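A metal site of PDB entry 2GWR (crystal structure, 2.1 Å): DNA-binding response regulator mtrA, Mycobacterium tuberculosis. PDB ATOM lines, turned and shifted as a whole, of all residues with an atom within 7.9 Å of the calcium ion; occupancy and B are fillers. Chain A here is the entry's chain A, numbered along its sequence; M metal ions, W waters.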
ATOM      1  N   VAL A  11     -18.786 -19.103  22.452  1.00  0.00           N
ATOM      2  CA  VAL A  11     -18.452 -17.731  22.782  1.00  0.00           C
ATOM      3  C   VAL A  11     -19.644 -17.131  23.538  1.00  0.00           C
ATOM      4  O   VAL A  11     -20.645 -16.680  22.952  1.00  0.00           O
ATOM      5  CB  VAL A  11     -18.051 -16.923  21.510  1.00  0.00           C
ATOM      6  CG1 VAL A  11     -17.523 -15.529  21.899  1.00  0.00           C
ATOM      7  CG2 VAL A  11     -16.977 -17.699  20.716  1.00  0.00           C
ATOM      8  N   ASP A  12     -19.547 -17.141  24.860  1.00  0.00           N
ATOM      9  CA  ASP A  12     -20.666 -16.723  25.692  1.00  0.00           C
ATOM     10  C   ASP A  12     -20.112 -16.338  27.042  1.00  0.00           C
ATOM     11  O   ASP A  12     -19.258 -17.054  27.589  1.00  0.00           O
ATOM     12  CB  ASP A  12     -21.688 -17.890  25.874  1.00  0.00           C
ATOM     13  CG  ASP A  12     -23.106 -17.376  26.242  1.00  0.00           C
ATOM     14  OD1 ASP A  12     -23.262 -16.726  27.315  1.00  0.00           O
ATOM     15  OD2 ASP A  12     -24.083 -17.591  25.439  1.00  0.00           O
ATOM     16  N   ASP A  13     -20.605 -15.235  27.599  1.00  0.00           N
ATOM     17  CA  ASP A  13     -20.154 -14.843  28.941  1.00  0.00           C
ATOM     18  C   ASP A  13     -21.021 -15.456  30.073  1.00  0.00           C
ATOM     19  O   ASP A  13     -20.726 -15.199  31.204  1.00  0.00           O
ATOM     20  CB  ASP A  13     -20.077 -13.329  29.127  1.00  0.00           C
ATOM     21  CG  ASP A  13     -21.428 -12.652  28.904  1.00  0.00           C
ATOM     22  OD1 ASP A  13     -22.125 -13.029  27.930  1.00  0.00           O
ATOM     23  OD2 ASP A  13     -21.774 -11.720  29.694  1.00  0.00           O
ATOM     24  N   ASP A  14     -22.074 -16.205  29.745  1.00  0.00           N
ATOM     25  CA  ASP A  14     -22.873 -16.927  30.759  1.00  0.00           C
ATOM     26  C   ASP A  14     -22.139 -18.242  31.105  1.00  0.00           C
ATOM     27  O   ASP A  14     -22.196 -19.227  30.365  1.00  0.00           O
ATOM     28  CB  ASP A  14     -24.289 -17.179  30.219  1.00  0.00           C
ATOM     29  CG  ASP A  14     -25.159 -18.025  31.172  1.00  0.00           C
ATOM     30  OD1 ASP A  14     -24.631 -18.603  32.155  1.00  0.00           O
ATOM     31  OD2 ASP A  14     -26.373 -18.088  30.928  1.00  0.00           O
ATOM     32  N   GLY A  36     -15.186 -16.010  26.780  1.00  0.00           N
ATOM     33  CA  GLY A  36     -16.249 -15.230  27.396  1.00  0.00           C
ATOM     34  C   GLY A  36     -16.300 -13.781  26.944  1.00  0.00           C
ATOM     35  O   GLY A  36     -17.184 -13.036  27.402  1.00  0.00           O
ATOM     36  N   ASP A  56     -22.906 -15.923  21.280  1.00  0.00           N
ATOM     37  CA  ASP A  56     -23.807 -15.022  21.991  1.00  0.00           C
ATOM     38  C   ASP A  56     -23.935 -13.639  21.304  1.00  0.00           C
ATOM     39  O   ASP A  56     -22.913 -12.983  20.991  1.00  0.00           O
ATOM     40  CB  ASP A  56     -23.238 -14.869  23.395  1.00  0.00           C
ATOM     41  CG  ASP A  56     -24.184 -14.271  24.396  1.00  0.00           C
ATOM     42  OD1 ASP A  56     -25.427 -14.245  24.179  1.00  0.00           O
ATOM     43  OD2 ASP A  56     -23.636 -13.875  25.451  1.00  0.00           O
ATOM     44  N   LEU A  57     -25.169 -13.174  21.081  1.00  0.00           N
ATOM     45  CA  LEU A  57     -25.381 -11.852  20.439  1.00  0.00           C
ATOM     46  C   LEU A  57     -24.858 -10.692  21.319  1.00  0.00           C
ATOM     47  O   LEU A  57     -24.200  -9.743  20.842  1.00  0.00           O
ATOM     48  CB  LEU A  57     -26.874 -11.630  20.107  1.00  0.00           C
ATOM     49  CG  LEU A  57     -27.297 -10.334  19.366  1.00  0.00           C
ATOM     50  CD1 LEU A  57     -26.433 -10.041  18.125  1.00  0.00           C
ATOM     51  CD2 LEU A  57     -28.794 -10.388  18.951  1.00  0.00           C
ATOM     52  N   MET A  58     -25.197 -10.735  22.609  1.00  0.00           N
ATOM     53  CA  MET A  58     -24.832  -9.700  23.552  1.00  0.00           C
ATOM     54  C   MET A  58     -23.589 -10.174  24.322  1.00  0.00           C
ATOM     55  O   MET A  58     -23.704 -10.969  25.206  1.00  0.00           O
ATOM     56  CB  MET A  58     -25.965  -9.454  24.542  1.00  0.00           C
ATOM     57  CG  MET A  58     -27.280  -9.081  23.930  1.00  0.00           C
ATOM     58  SD  MET A  58     -27.290  -7.343  23.028  1.00  0.00           S
ATOM     59  CE  MET A  58     -26.279  -6.301  24.240  1.00  0.00           C
ATOM     60  N   LEU A  59     -22.386  -9.722  23.977  1.00  0.00           N
ATOM     61  CA  LEU A  59     -21.193 -10.193  24.682  1.00  0.00           C
ATOM     62  C   LEU A  59     -20.414  -9.036  25.232  1.00  0.00           C
ATOM     63  O   LEU A  59     -20.454  -7.965  24.659  1.00  0.00           O
ATOM     64  CB  LEU A  59     -20.245 -10.878  23.715  1.00  0.00           C
ATOM     65  CG  LEU A  59     -20.189 -12.329  23.340  1.00  0.00           C
ATOM     66  CD1 LEU A  59     -19.066 -12.383  22.277  1.00  0.00           C
ATOM     67  CD2 LEU A  59     -19.863 -13.192  24.527  1.00  0.00           C
ATOM     68  N   PRO A  60     -19.636  -9.262  26.307  1.00  0.00           N
ATOM     69  CA  PRO A  60     -18.637  -8.243  26.688  1.00  0.00           C
ATOM     70  C   PRO A  60     -17.552  -8.086  25.615  1.00  0.00           C
ATOM     71  O   PRO A  60     -17.209  -9.022  24.853  1.00  0.00           O
ATOM     72  CB  PRO A  60     -17.970  -8.849  27.940  1.00  0.00           C
ATOM     73  CG  PRO A  60     -18.819 -10.039  28.325  1.00  0.00           C
ATOM     74  CD  PRO A  60     -19.512 -10.498  27.076  1.00  0.00           C
ATOM     75  N   LEU A  82     -26.649 -17.105  19.381  1.00  0.00           N
ATOM     76  CA  LEU A  82     -27.580 -17.328  20.505  1.00  0.00           C
ATOM     77  C   LEU A  82     -28.200 -16.001  20.940  1.00  0.00           C
ATOM     78  O   LEU A  82     -27.496 -15.052  21.305  1.00  0.00           O
ATOM     79  CB  LEU A  82     -26.836 -17.957  21.687  1.00  0.00           C
ATOM     80  CG  LEU A  82     -25.864 -19.077  21.292  1.00  0.00           C
ATOM     81  CD1 LEU A  82     -25.177 -19.630  22.568  1.00  0.00           C
ATOM     82  CD2 LEU A  82     -26.563 -20.173  20.480  1.00  0.00           C
ATOM     83  N   ALA A  84     -31.608 -13.706  22.872  1.00  0.00           N
ATOM     84  CA  ALA A  84     -32.531 -13.816  24.018  1.00  0.00           C
ATOM     85  C   ALA A  84     -33.493 -12.696  23.839  1.00  0.00           C
ATOM     86  O   ALA A  84     -33.176 -11.732  23.140  1.00  0.00           O
ATOM     87  CB  ALA A  84     -31.783 -13.678  25.339  1.00  0.00           C
ATOM     88  N   THR A  86     -34.256 -10.495  25.720  1.00  0.00           N
ATOM     89  CA  THR A  86     -33.724  -9.266  26.293  1.00  0.00           C
ATOM     90  C   THR A  86     -32.727  -8.516  25.383  1.00  0.00           C
ATOM     91  O   THR A  86     -32.389  -7.379  25.664  1.00  0.00           O
ATOM     92  CB  THR A  86     -33.112  -9.541  27.661  1.00  0.00           C
ATOM     93  OG1 THR A  86     -32.129 -10.576  27.544  1.00  0.00           O
ATOM     94  CG2 THR A  86     -34.228  -9.942  28.658  1.00  0.00           C
ATOM     95  N   ASP A  87     -32.274  -9.153  24.305  1.00  0.00           N
ATOM     96  CA  ASP A  87     -31.240  -8.568  23.453  1.00  0.00           C
ATOM     97  C   ASP A  87     -31.637  -7.168  23.059  1.00  0.00           C
ATOM     98  O   ASP A  87     -32.797  -6.923  22.750  1.00  0.00           O
ATOM     99  CB  ASP A  87     -31.049  -9.396  22.192  1.00  0.00           C
ATOM    100  CG  ASP A  87     -30.457 -10.780  22.480  1.00  0.00           C
ATOM    101  OD1 ASP A  87     -29.896 -10.990  23.582  1.00  0.00           O
ATOM    102  OD2 ASP A  87     -30.556 -11.641  21.582  1.00  0.00           O
ATOM    103  N   LYS A 105     -32.616 -18.148  23.298  1.00  0.00           N
ATOM    104  CA  LYS A 105     -32.526 -18.667  24.662  1.00  0.00           C
ATOM    105  C   LYS A 105     -33.856 -18.340  25.344  1.00  0.00           C
ATOM    106  O   LYS A 105     -34.455 -17.287  25.089  1.00  0.00           O
ATOM    107  CB  LYS A 105     -31.415 -17.980  25.460  1.00  0.00           C
ATOM    108  CG  LYS A 105     -29.999 -18.018  24.866  1.00  0.00           C
ATOM    109  CD  LYS A 105     -29.087 -16.958  25.591  1.00  0.00           C
ATOM    110  CE  LYS A 105     -27.596 -17.108  25.291  1.00  0.00           C
ATOM    111  NZ  LYS A 105     -26.711 -16.235  26.163  1.00  0.00           N
HETATM  112 CA    CA M   1     -24.634 -12.478  27.010  1.00  0.00          CA
HETATM  113  O   HOH W   1     -24.977 -14.813  28.130  1.00  0.00           O
HETATM  114  O   HOH W   2     -27.653 -11.837  26.925  1.00  0.00           O
HETATM  115  O   HOH W   3     -24.096 -10.605  28.831  1.00  0.00           O
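The calcium ion is bound by the side-chain carboxylate (OD2) of Asp 56, at 2.3 Å.
The calcium ion is bound by the backbone carbonyl oxygen (O) of Met 58, at 2.5 Å.
Water W1 binds the calcium ion (2.6 Å).
Water W3 is bound to the calcium ion, 2.7 Å away.
OD1 of Asp 13 is bound to the calcium ion, at 2.7 Å.
The calcium ion has five donor atoms within binding distance.
Slightly farther from the calcium ion lies water W2 (3.1 Å).
Water W1 lies within hydrogen-bond range of OD1 of Asp 12 and NZ of Lys 105.
The backbone NH (N) of Asp 56 is in hydrogen-bond range of the backbone carbonyl oxygen (O) of Val 11, 2.9 Å away.
OD1 of Asp 56 is in salt-bridge range of NZ of Lys 105.
Along chain A the residues within 4 Å of the calcium ion span positions 13 to 58.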
